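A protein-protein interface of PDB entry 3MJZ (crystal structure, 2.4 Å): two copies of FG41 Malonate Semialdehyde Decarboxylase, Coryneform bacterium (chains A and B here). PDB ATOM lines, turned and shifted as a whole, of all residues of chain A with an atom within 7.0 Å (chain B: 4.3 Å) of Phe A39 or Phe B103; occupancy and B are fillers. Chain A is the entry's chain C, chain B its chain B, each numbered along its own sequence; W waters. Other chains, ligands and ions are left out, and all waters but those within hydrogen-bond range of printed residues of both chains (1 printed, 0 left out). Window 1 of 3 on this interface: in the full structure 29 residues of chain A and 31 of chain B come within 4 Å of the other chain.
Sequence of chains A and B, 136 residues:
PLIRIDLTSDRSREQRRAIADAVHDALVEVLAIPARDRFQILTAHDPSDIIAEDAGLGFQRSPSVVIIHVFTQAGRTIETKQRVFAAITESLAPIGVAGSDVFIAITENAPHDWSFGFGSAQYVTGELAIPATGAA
NH1 of Arg B61 is in hydrogen-bond range of O of Glu B53, at 2.5 Å.
The backbone carbonyl oxygen (O) of Val B102 lies within hydrogen-bond range of the guanidinium group (NH2) of Arg B61, 3.0 Å away.
The backbone carbonyl oxygen (O) of Val B66 lies within hydrogen-bond range of the backbone NH (N) of Phe B103.
The backbone carbonyl oxygen (O) of Phe B103 sits at hydrogen-bond distance from the backbone NH (N) of Ile B68 (2.7 Å).
N of Ile A3 sits at hydrogen-bond distance from O of Phe A39, 2.8 Å away.
The backbone carbonyl oxygen of Ile A3 lies within hydrogen-bond range of the backbone NH of Ile A41.
O of Arg A38 touches CA of Ala B52, 3.4 Å away.
Phe A39 touches Ile B51 (CA to O, 3.1 Å).
CD2 of Phe A39 touches CA of Ala B52, at 3.6 Å.
Phe A39 touches Phe B103 (CD2 to CE1, 3.4 Å).
Ile B67 touches Ile A41.
Phe B103 touches Trp A114.
Phe B103 touches Ser A115 (CA to O, 3.5 Å).
O of Val B102 touches O of Phe A116, 3.7 Å away.
Phe A116 touches Phe B103 (CD1 to CE1, 3.6 Å).
Leu A128 touches Ala B55.
The backbone carbonyl oxygen (O) of Ile B51 is in hydrogen-bond range of the backbone NH (N) of Gln A40, at 2.7 Å.
NH1 of Arg A36 is in salt-bridge range of OE1 of Glu B53.
The backbone carbonyl oxygen of Arg A38 sits at hydrogen-bond distance from the backbone NH of Glu B53.
The side-chain carboxylate of Asp B54 lies within salt-bridge range of the guanidinium group of Arg A36 (2.4 Å).
O of Arg A36 lies within hydrogen-bond range of N of Ala B55 (3.0 Å).
The backbone carbonyl oxygen (O) of Phe A116 lies within hydrogen-bond range of the guanidinium group (NH2) of Arg B61 (2.6 Å).
The backbone NH of Gly A117 lies close to the backbone carbonyl oxygen of Val B102 (3.5 Å).
The backbone carbonyl oxygen (O) of Ile B104 is in hydrogen-bond range of the backbone NH (N) of Ser A115 (2.8 Å).
The backbone carbonyl oxygen (O) of Ile B51 lies close to the backbone carbonyl oxygen (O) of Arg A38, 3.2 Å away.
No position is printed for both chains.
Among the printed residues, 24 pairs touch across the chains.
Among the printed residues, Asp or Glu carboxylates within 4 Å of a Lys or Arg side-chain nitrogen of the other chain: Arg A36 with Glu B53 and Arg A36 with Asp B54.
Of the printed residues of chain B, Phe A39 touches Ile B51, Ala B52, Glu B53, Arg B61 and Phe B103.
Of the printed residues of chain B, Ser A115 touches Phe B103 (3.5 Å) and Ile B104 (2.8 Å).
Of the printed residues of chain B, Ile A41 touches Ile B67 (3.8 Å).
Of the printed residues of chain B, Leu A128 touches Ala B55 (3.99 Å).
Printed residues of chain A within 4 Å of Ile B104: Trp A114 (3.5 Å) and Ser A115 (2.8 Å).
Val B66 touches none of the printed residues of chain A.
The nearest residue of chain B that does not touch Phe A39 is Asp B54 (4.1 Å).
Water W1 bridges O of Ile B67 (3.0 Å) and NH2 of Arg A4 (3.0 Å).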
ATOM      1  N   PRO A   1      13.391  18.642   0.612  1.00  0.00           N
ATOM      2  CA  PRO A   1      14.776  18.849   0.177  1.00  0.00           C
ATOM      3  C   PRO A   1      15.683  18.873   1.377  1.00  0.00           C
ATOM      4  O   PRO A   1      15.182  19.142   2.459  1.00  0.00           O
ATOM      5  CB  PRO A   1      14.751  20.251  -0.464  1.00  0.00           C
ATOM      6  CG  PRO A   1      13.483  20.892   0.071  1.00  0.00           C
ATOM      7  CD  PRO A   1      12.515  19.772   0.233  1.00  0.00           C
ATOM      8  N   LEU A   2      16.980  18.596   1.180  1.00  0.00           N
ATOM      9  CA  LEU A   2      18.030  18.703   2.213  1.00  0.00           C
ATOM     10  C   LEU A   2      18.877  19.945   1.880  1.00  0.00           C
ATOM     11  O   LEU A   2      19.446  20.039   0.793  1.00  0.00           O
ATOM     12  CB  LEU A   2      18.903  17.436   2.235  1.00  0.00           C
ATOM     13  CG  LEU A   2      19.881  17.036   3.387  1.00  0.00           C
ATOM     14  CD1 LEU A   2      21.340  17.497   3.193  1.00  0.00           C
ATOM     15  CD2 LEU A   2      19.403  17.371   4.827  1.00  0.00           C
ATOM     16  N   ILE A   3      18.940  20.916   2.782  1.00  0.00           N
ATOM     17  CA  ILE A   3      19.712  22.113   2.476  1.00  0.00           C
ATOM     18  C   ILE A   3      20.932  22.136   3.378  1.00  0.00           C
ATOM     19  O   ILE A   3      20.826  21.977   4.574  1.00  0.00           O
ATOM     20  CB  ILE A   3      18.847  23.437   2.545  1.00  0.00           C
ATOM     21  CG1 ILE A   3      17.575  23.281   1.718  1.00  0.00           C
ATOM     22  CG2 ILE A   3      19.605  24.677   2.037  1.00  0.00           C
ATOM     23  CD1 ILE A   3      16.479  22.686   2.520  1.00  0.00           C
ATOM     24  N   ARG A   4      22.093  22.266   2.759  1.00  0.00           N
ATOM     25  CA  ARG A   4      23.334  22.520   3.458  1.00  0.00           C
ATOM     26  C   ARG A   4      23.647  24.014   3.349  1.00  0.00           C
ATOM     27  O   ARG A   4      23.810  24.543   2.265  1.00  0.00           O
ATOM     28  CB  ARG A   4      24.457  21.683   2.852  1.00  0.00           C
ATOM     29  CG  ARG A   4      24.410  20.226   3.282  1.00  0.00           C
ATOM     30  CD  ARG A   4      25.626  19.461   2.825  1.00  0.00           C
ATOM     31  NE  ARG A   4      25.305  18.050   2.910  1.00  0.00           N
ATOM     32  CZ  ARG A   4      25.660  17.230   3.895  1.00  0.00           C
ATOM     33  NH1 ARG A   4      26.417  17.649   4.915  1.00  0.00           N
ATOM     34  NH2 ARG A   4      25.238  15.979   3.847  1.00  0.00           N
ATOM     35  N   HIS A  24      14.176  28.492   4.175  1.00  0.00           N
ATOM     36  CA  HIS A  24      13.014  27.624   4.162  1.00  0.00           C
ATOM     37  C   HIS A  24      11.761  28.305   3.651  1.00  0.00           C
ATOM     38  O   HIS A  24      11.116  27.766   2.784  1.00  0.00           O
ATOM     39  CB  HIS A  24      12.748  26.980   5.517  1.00  0.00           C
ATOM     40  CG  HIS A  24      11.586  26.036   5.502  1.00  0.00           C
ATOM     41  ND1 HIS A  24      11.609  24.840   4.814  1.00  0.00           N
ATOM     42  CD2 HIS A  24      10.362  26.117   6.080  1.00  0.00           C
ATOM     43  CE1 HIS A  24      10.451  24.221   4.975  1.00  0.00           C
ATOM     44  NE2 HIS A  24       9.675  24.972   5.743  1.00  0.00           N
ATOM     45  N   LEU A  27      11.639  28.499  -0.167  1.00  0.00           N
ATOM     46  CA  LEU A  27      11.443  27.171  -0.753  1.00  0.00           C
ATOM     47  C   LEU A  27       9.982  26.745  -0.665  1.00  0.00           C
ATOM     48  O   LEU A  27       9.441  26.201  -1.612  1.00  0.00           O
ATOM     49  CB  LEU A  27      12.333  26.131  -0.047  1.00  0.00           C
ATOM     50  CG  LEU A  27      13.745  25.750  -0.530  1.00  0.00           C
ATOM     51  CD1 LEU A  27      14.681  26.884  -0.452  1.00  0.00           C
ATOM     52  CD2 LEU A  27      14.308  24.651   0.340  1.00  0.00           C
ATOM     53  N   ARG A  36       6.163  21.765   6.847  1.00  0.00           N
ATOM     54  CA  ARG A  36       7.072  21.035   7.741  1.00  0.00           C
ATOM     55  C   ARG A  36       8.205  20.241   7.026  1.00  0.00           C
ATOM     56  O   ARG A  36       8.940  19.477   7.659  1.00  0.00           O
ATOM     57  CB  ARG A  36       6.277  20.159   8.723  1.00  0.00           C
ATOM     58  CG  ARG A  36       5.397  20.919   9.733  1.00  0.00           C
ATOM     59  CD  ARG A  36       4.963  20.008  10.892  1.00  0.00           C
ATOM     60  NE  ARG A  36       5.648  20.268  12.173  1.00  0.00           N
ATOM     61  CZ  ARG A  36       6.784  19.694  12.564  1.00  0.00           C
ATOM     62  NH1 ARG A  36       7.399  18.827  11.777  1.00  0.00           N
ATOM     63  NH2 ARG A  36       7.331  19.989  13.736  1.00  0.00           N
ATOM     64  N   ASP A  37       8.345  20.437   5.715  1.00  0.00           N
ATOM     65  CA  ASP A  37       9.330  19.719   4.914  1.00  0.00           C
ATOM     66  C   ASP A  37      10.690  20.431   4.998  1.00  0.00           C
ATOM     67  O   ASP A  37      11.300  20.793   3.981  1.00  0.00           O
ATOM     68  CB  ASP A  37       8.847  19.546   3.467  1.00  0.00           C
ATOM     69  CG  ASP A  37       9.730  18.580   2.648  1.00  0.00           C
ATOM     70  OD1 ASP A  37      10.713  18.031   3.213  1.00  0.00           O
ATOM     71  OD2 ASP A  37       9.442  18.389   1.431  1.00  0.00           O
ATOM     72  N   ARG A  38      11.149  20.567   6.244  1.00  0.00           N
ATOM     73  CA  ARG A  38      12.301  21.351   6.617  1.00  0.00           C
ATOM     74  C   ARG A  38      13.477  20.511   7.144  1.00  0.00           C
ATOM     75  O   ARG A  38      13.432  19.921   8.242  1.00  0.00           O
ATOM     76  CB  ARG A  38      11.891  22.382   7.647  1.00  0.00           C
ATOM     77  CG  ARG A  38      13.042  23.179   8.117  1.00  0.00           C
ATOM     78  CD  ARG A  38      12.553  24.371   8.813  1.00  0.00           C
ATOM     79  NE  ARG A  38      13.677  25.261   9.004  1.00  0.00           N
ATOM     80  CZ  ARG A  38      13.588  26.456   9.548  1.00  0.00           C
ATOM     81  NH1 ARG A  38      12.403  26.899   9.940  1.00  0.00           N
ATOM     82  NH2 ARG A  38      14.686  27.186   9.707  1.00  0.00           N
ATOM     83  N   PHE A  39      14.514  20.457   6.315  1.00  0.00           N
ATOM     84  CA  PHE A  39      15.650  19.601   6.554  1.00  0.00           C
ATOM     85  C   PHE A  39      16.881  20.359   6.169  1.00  0.00           C
ATOM     86  O   PHE A  39      17.188  20.503   4.984  1.00  0.00           O
ATOM     87  CB  PHE A  39      15.502  18.281   5.795  1.00  0.00           C
ATOM     88  CG  PHE A  39      14.295  17.521   6.204  1.00  0.00           C
ATOM     89  CD1 PHE A  39      13.163  17.502   5.400  1.00  0.00           C
ATOM     90  CD2 PHE A  39      14.260  16.858   7.430  1.00  0.00           C
ATOM     91  CE1 PHE A  39      12.026  16.807   5.809  1.00  0.00           C
ATOM     92  CE2 PHE A  39      13.122  16.176   7.826  1.00  0.00           C
ATOM     93  CZ  PHE A  39      12.015  16.169   7.028  1.00  0.00           C
ATOM     94  N   GLN A  40      17.552  20.849   7.210  1.00  0.00           N
ATOM     95  CA  GLN A  40      18.646  21.799   7.104  1.00  0.00           C
ATOM     96  C   GLN A  40      19.796  21.468   8.044  1.00  0.00           C
ATOM     97  O   GLN A  40      19.598  21.181   9.217  1.00  0.00           O
ATOM     98  CB  GLN A  40      18.138  23.214   7.394  1.00  0.00           C
ATOM     99  CG  GLN A  40      17.040  23.705   6.455  1.00  0.00           C
ATOM    100  CD  GLN A  40      16.546  25.091   6.837  1.00  0.00           C
ATOM    101  OE1 GLN A  40      16.476  25.425   8.026  1.00  0.00           O
ATOM    102  NE2 GLN A  40      16.217  25.917   5.831  1.00  0.00           N
ATOM    103  N   ILE A  41      21.004  21.513   7.494  1.00  0.00           N
ATOM    104  CA  ILE A  41      22.240  21.451   8.258  1.00  0.00           C
ATOM    105  C   ILE A  41      23.005  22.785   8.112  1.00  0.00           C
ATOM    106  O   ILE A  41      23.455  23.129   7.019  1.00  0.00           O
ATOM    107  CB  ILE A  41      23.101  20.229   7.842  1.00  0.00           C
ATOM    108  CG1 ILE A  41      22.284  18.954   8.004  1.00  0.00           C
ATOM    109  CG2 ILE A  41      24.387  20.138   8.693  1.00  0.00           C
ATOM    110  CD1 ILE A  41      22.515  17.967   6.923  1.00  0.00           C
ATOM    111  N   PHE A  71      19.678  20.075  -2.056  1.00  0.00           N
ATOM    112  CA  PHE A  71      19.537  18.672  -2.473  1.00  0.00           C
ATOM    113  C   PHE A  71      18.054  18.321  -2.575  1.00  0.00           C
ATOM    114  O   PHE A  71      17.327  18.311  -1.572  1.00  0.00           O
ATOM    115  CB  PHE A  71      20.242  17.723  -1.494  1.00  0.00           C
ATOM    116  CG  PHE A  71      21.748  17.833  -1.518  1.00  0.00           C
ATOM    117  CD1 PHE A  71      22.415  18.628  -0.600  1.00  0.00           C
ATOM    118  CD2 PHE A  71      22.502  17.130  -2.459  1.00  0.00           C
ATOM    119  CE1 PHE A  71      23.816  18.728  -0.608  1.00  0.00           C
ATOM    120  CE2 PHE A  71      23.907  17.226  -2.478  1.00  0.00           C
ATOM    121  CZ  PHE A  71      24.558  18.036  -1.538  1.00  0.00           C
ATOM    122  N   TRP A 114      15.018   8.887  -0.595  1.00  0.00           N
ATOM    123  CA  TRP A 114      14.742   9.615   0.648  1.00  0.00           C
ATOM    124  C   TRP A 114      14.115   8.723   1.693  1.00  0.00           C
ATOM    125  O   TRP A 114      13.208   7.940   1.396  1.00  0.00           O
ATOM    126  CB  TRP A 114      13.782  10.787   0.402  1.00  0.00           C
ATOM    127  CG  TRP A 114      14.290  11.808  -0.519  1.00  0.00           C
ATOM    128  CD1 TRP A 114      14.072  11.876  -1.848  1.00  0.00           C
ATOM    129  CD2 TRP A 114      15.129  12.905  -0.184  1.00  0.00           C
ATOM    130  NE1 TRP A 114      14.718  12.971  -2.384  1.00  0.00           N
ATOM    131  CE2 TRP A 114      15.376  13.623  -1.375  1.00  0.00           C
ATOM    132  CE3 TRP A 114      15.699  13.365   1.012  1.00  0.00           C
ATOM    133  CZ2 TRP A 114      16.181  14.774  -1.406  1.00  0.00           C
ATOM    134  CZ3 TRP A 114      16.480  14.524   0.978  1.00  0.00           C
ATOM    135  CH2 TRP A 114      16.719  15.202  -0.214  1.00  0.00           C
ATOM    136  N   SER A 115      14.630   8.838   2.913  1.00  0.00           N
ATOM    137  CA  SER A 115      14.059   8.231   4.088  1.00  0.00           C
ATOM    138  C   SER A 115      13.939   9.276   5.186  1.00  0.00           C
ATOM    139  O   SER A 115      14.921   9.744   5.713  1.00  0.00           O
ATOM    140  CB  SER A 115      14.935   7.090   4.562  1.00  0.00           C
ATOM    141  OG  SER A 115      14.298   6.435   5.633  1.00  0.00           O
ATOM    142  N   PHE A 116      12.709   9.633   5.507  1.00  0.00           N
ATOM    143  CA  PHE A 116      12.399  10.652   6.493  1.00  0.00           C
ATOM    144  C   PHE A 116      12.426  10.171   7.931  1.00  0.00           C
ATOM    145  O   PHE A 116      12.277  10.965   8.861  1.00  0.00           O
ATOM    146  CB  PHE A 116      11.022  11.236   6.169  1.00  0.00           C
ATOM    147  CG  PHE A 116      10.986  11.979   4.848  1.00  0.00           C
ATOM    148  CD1 PHE A 116      11.302  13.332   4.791  1.00  0.00           C
ATOM    149  CD2 PHE A 116      10.644  11.318   3.671  1.00  0.00           C
ATOM    150  CE1 PHE A 116      11.285  14.018   3.595  1.00  0.00           C
ATOM    151  CE2 PHE A 116      10.624  11.990   2.468  1.00  0.00           C
ATOM    152  CZ  PHE A 116      10.953  13.362   2.437  1.00  0.00           C
ATOM    153  N   GLY A 117      12.571   8.863   8.112  1.00  0.00           N
ATOM    154  CA  GLY A 117      12.626   8.268   9.438  1.00  0.00           C
ATOM    155  C   GLY A 117      12.077   6.859   9.424  1.00  0.00           C
ATOM    156  O   GLY A 117      11.363   6.475   8.487  1.00  0.00           O
ATOM    157  N   PHE A 118      12.419   6.089  10.462  1.00  0.00           N
ATOM    158  CA  PHE A 118      11.835   4.767  10.710  1.00  0.00           C
ATOM    159  C   PHE A 118      12.303   3.707   9.716  1.00  0.00           C
ATOM    160  O   PHE A 118      11.741   2.613   9.670  1.00  0.00           O
ATOM    161  CB  PHE A 118      10.300   4.842  10.759  1.00  0.00           C
ATOM    162  CG  PHE A 118       9.785   5.872  11.709  1.00  0.00           C
ATOM    163  CD1 PHE A 118       9.337   7.093  11.244  1.00  0.00           C
ATOM    164  CD2 PHE A 118       9.809   5.642  13.084  1.00  0.00           C
ATOM    165  CE1 PHE A 118       8.870   8.062  12.113  1.00  0.00           C
ATOM    166  CE2 PHE A 118       9.357   6.619  13.979  1.00  0.00           C
ATOM    167  CZ  PHE A 118       8.868   7.835  13.482  1.00  0.00           C
ATOM    168  N   LEU A 128       3.850   9.682   1.725  1.00  0.00           N
ATOM    169  CA  LEU A 128       4.124  11.071   1.469  1.00  0.00           C
ATOM    170  C   LEU A 128       3.976  11.275  -0.014  1.00  0.00           C
ATOM    171  O   LEU A 128       4.664  10.652  -0.807  1.00  0.00           O
ATOM    172  CB  LEU A 128       5.557  11.423   1.885  1.00  0.00           C
ATOM    173  CG  LEU A 128       5.951  12.724   2.586  1.00  0.00           C
ATOM    174  CD1 LEU A 128       7.452  12.834   2.581  1.00  0.00           C
ATOM    175  CD2 LEU A 128       5.407  13.944   1.963  1.00  0.00           C
ATOM    176  N   ILE B  51      18.199  21.009  11.677  1.00  0.00           N
ATOM    177  CA  ILE B  51      16.775  21.210  11.665  1.00  0.00           C
ATOM    178  C   ILE B  51      16.163  20.153  10.774  1.00  0.00           C
ATOM    179  O   ILE B  51      16.385  20.119   9.557  1.00  0.00           O
ATOM    180  CB  ILE B  51      16.396  22.615  11.191  1.00  0.00           C
ATOM    181  CG1 ILE B  51      17.186  23.668  11.988  1.00  0.00           C
ATOM    182  CG2 ILE B  51      14.873  22.814  11.302  1.00  0.00           C
ATOM    183  CD1 ILE B  51      17.199  25.050  11.384  1.00  0.00           C
ATOM    184  N   ALA B  52      15.402  19.278  11.416  1.00  0.00           N
ATOM    185  CA  ALA B  52      14.809  18.109  10.789  1.00  0.00           C
ATOM    186  C   ALA B  52      13.441  17.929  11.408  1.00  0.00           C
ATOM    187  O   ALA B  52      13.334  17.480  12.560  1.00  0.00           O
ATOM    188  CB  ALA B  52      15.670  16.867  11.041  1.00  0.00           C
ATOM    189  N   GLU B  53      12.412  18.317  10.647  1.00  0.00           N
ATOM    190  CA  GLU B  53      11.021  18.125  11.044  1.00  0.00           C
ATOM    191  C   GLU B  53      10.413  16.793  10.476  1.00  0.00           C
ATOM    192  O   GLU B  53      11.084  15.778  10.528  1.00  0.00           O
ATOM    193  CB  GLU B  53      10.233  19.385  10.698  1.00  0.00           C
ATOM    194  CG  GLU B  53      10.751  20.643  11.399  1.00  0.00           C
ATOM    195  CD  GLU B  53       9.915  21.856  11.069  1.00  0.00           C
ATOM    196  OE1 GLU B  53       9.271  21.848  10.005  1.00  0.00           O
ATOM    197  OE2 GLU B  53       9.892  22.832  11.855  1.00  0.00           O
ATOM    198  N   ASP B  54       9.177  16.767   9.952  1.00  0.00           N
ATOM    199  CA  ASP B  54       8.571  15.488   9.541  1.00  0.00           C
ATOM    200  C   ASP B  54       7.910  15.501   8.168  1.00  0.00           C
ATOM    201  O   ASP B  54       7.384  14.484   7.708  1.00  0.00           O
ATOM    202  CB  ASP B  54       7.550  15.007  10.581  1.00  0.00           C
ATOM    203  CG  ASP B  54       6.377  15.969  10.743  1.00  0.00           C
ATOM    204  OD1 ASP B  54       6.474  17.129  10.274  1.00  0.00           O
ATOM    205  OD2 ASP B  54       5.348  15.579  11.324  1.00  0.00           O
ATOM    206  N   ALA B  55       7.895  16.654   7.518  1.00  0.00           N
ATOM    207  CA  ALA B  55       7.243  16.780   6.203  1.00  0.00           C
ATOM    208  C   ALA B  55       5.728  16.576   6.298  1.00  0.00           C
ATOM    209  O   ALA B  55       5.079  16.234   5.314  1.00  0.00           O
ATOM    210  CB  ALA B  55       7.879  15.817   5.190  1.00  0.00           C
ATOM    211  N   ARG B  61      10.730  14.285  16.612  1.00  0.00           N
ATOM    212  CA  ARG B  61      12.069  13.743  16.718  1.00  0.00           C
ATOM    213  C   ARG B  61      12.625  14.344  17.965  1.00  0.00           C
ATOM    214  O   ARG B  61      12.072  15.335  18.464  1.00  0.00           O
ATOM    215  CB  ARG B  61      12.921  14.167  15.510  1.00  0.00           C
ATOM    216  CG  ARG B  61      12.141  14.243  14.216  1.00  0.00           C
ATOM    217  CD  ARG B  61      13.035  14.606  13.031  1.00  0.00           C
ATOM    218  NE  ARG B  61      13.583  13.418  12.388  1.00  0.00           N
ATOM    219  CZ  ARG B  61      13.260  12.957  11.182  1.00  0.00           C
ATOM    220  NH1 ARG B  61      12.388  13.591  10.399  1.00  0.00           N
ATOM    221  NH2 ARG B  61      13.836  11.834  10.757  1.00  0.00           N
ATOM    222  N   VAL B  66      20.199  12.437  13.554  1.00  0.00           N
ATOM    223  CA  VAL B  66      21.331  11.980  12.738  1.00  0.00           C
ATOM    224  C   VAL B  66      20.919  11.986  11.277  1.00  0.00           C
ATOM    225  O   VAL B  66      19.952  11.329  10.904  1.00  0.00           O
ATOM    226  CB  VAL B  66      21.799  10.564  13.145  1.00  0.00           C
ATOM    227  CG1 VAL B  66      22.938  10.081  12.230  1.00  0.00           C
ATOM    228  CG2 VAL B  66      22.229  10.541  14.638  1.00  0.00           C
ATOM    229  N   ILE B  67      21.619  12.772  10.463  1.00  0.00           N
ATOM    230  CA  ILE B  67      21.362  12.856   9.040  1.00  0.00           C
ATOM    231  C   ILE B  67      22.485  12.131   8.308  1.00  0.00           C
ATOM    232  O   ILE B  67      23.663  12.469   8.450  1.00  0.00           O
ATOM    233  CB  ILE B  67      21.254  14.303   8.570  1.00  0.00           C
ATOM    234  CG1 ILE B  67      19.970  14.899   9.114  1.00  0.00           C
ATOM    235  CG2 ILE B  67      21.258  14.382   7.023  1.00  0.00           C
ATOM    236  CD1 ILE B  67      20.129  16.298   9.589  1.00  0.00           C
ATOM    237  N   ILE B  68      22.091  11.124   7.536  1.00  0.00           N
ATOM    238  CA  ILE B  68      23.009  10.291   6.780  1.00  0.00           C
ATOM    239  C   ILE B  68      22.739  10.494   5.303  1.00  0.00           C
ATOM    240  O   ILE B  68      21.633  10.229   4.837  1.00  0.00           O
ATOM    241  CB  ILE B  68      22.831   8.815   7.173  1.00  0.00           C
ATOM    242  CG1 ILE B  68      23.139   8.655   8.674  1.00  0.00           C
ATOM    243  CG2 ILE B  68      23.687   7.873   6.267  1.00  0.00           C
ATOM    244  CD1 ILE B  68      22.375   7.519   9.317  1.00  0.00           C
ATOM    245  N   ASP B 101      14.629   9.778  14.647  1.00  0.00           N
ATOM    246  CA  ASP B 101      15.797  10.714  14.569  1.00  0.00           C
ATOM    247  C   ASP B 101      16.786  10.462  13.414  1.00  0.00           C
ATOM    248  O   ASP B 101      17.842  11.094  13.362  1.00  0.00           O
ATOM    249  CB  ASP B 101      16.580  10.687  15.891  1.00  0.00           C
ATOM    250  CG  ASP B 101      15.731  11.033  17.083  1.00  0.00           C
ATOM    251  OD1 ASP B 101      14.647  11.635  16.887  1.00  0.00           O
ATOM    252  OD2 ASP B 101      16.163  10.731  18.224  1.00  0.00           O
ATOM    253  N   VAL B 102      16.448   9.561  12.498  1.00  0.00           N
ATOM    254  CA  VAL B 102      17.319   9.207  11.383  1.00  0.00           C
ATOM    255  C   VAL B 102      16.724   9.764  10.100  1.00  0.00           C
ATOM    256  O   VAL B 102      15.536   9.547   9.814  1.00  0.00           O
ATOM    257  CB  VAL B 102      17.447   7.661  11.231  1.00  0.00           C
ATOM    258  CG1 VAL B 102      18.416   7.294  10.102  1.00  0.00           C
ATOM    259  CG2 VAL B 102      17.847   6.968  12.578  1.00  0.00           C
ATOM    260  N   PHE B 103      17.550  10.485   9.336  1.00  0.00           N
ATOM    261  CA  PHE B 103      17.173  10.992   8.010  1.00  0.00           C
ATOM    262  C   PHE B 103      18.233  10.585   6.987  1.00  0.00           C
ATOM    263  O   PHE B 103      19.417  10.805   7.204  1.00  0.00           O
ATOM    264  CB  PHE B 103      17.024  12.515   8.073  1.00  0.00           C
ATOM    265  CG  PHE B 103      16.562  13.154   6.793  1.00  0.00           C
ATOM    266  CD1 PHE B 103      15.239  13.474   6.619  1.00  0.00           C
ATOM    267  CD2 PHE B 103      17.469  13.495   5.801  1.00  0.00           C
ATOM    268  CE1 PHE B 103      14.803  14.093   5.466  1.00  0.00           C
ATOM    269  CE2 PHE B 103      17.041  14.111   4.632  1.00  0.00           C
ATOM    270  CZ  PHE B 103      15.703  14.407   4.465  1.00  0.00           C
ATOM    271  N   ILE B 104      17.805   9.981   5.880  1.00  0.00           N
ATOM    272  CA  ILE B 104      18.716   9.473   4.848  1.00  0.00           C
ATOM    273  C   ILE B 104      18.365  10.027   3.472  1.00  0.00           C
ATOM    274  O   ILE B 104      17.184  10.065   3.099  1.00  0.00           O
ATOM    275  CB  ILE B 104      18.703   7.935   4.764  1.00  0.00           C
ATOM    276  CG1 ILE B 104      18.743   7.316   6.170  1.00  0.00           C
ATOM    277  CG2 ILE B 104      19.890   7.461   3.988  1.00  0.00           C
ATOM    278  CD1 ILE B 104      18.131   5.897   6.283  1.00  0.00           C
HETATM  279  O   HOH W   1      24.615  14.438   6.384  1.00  0.00           O
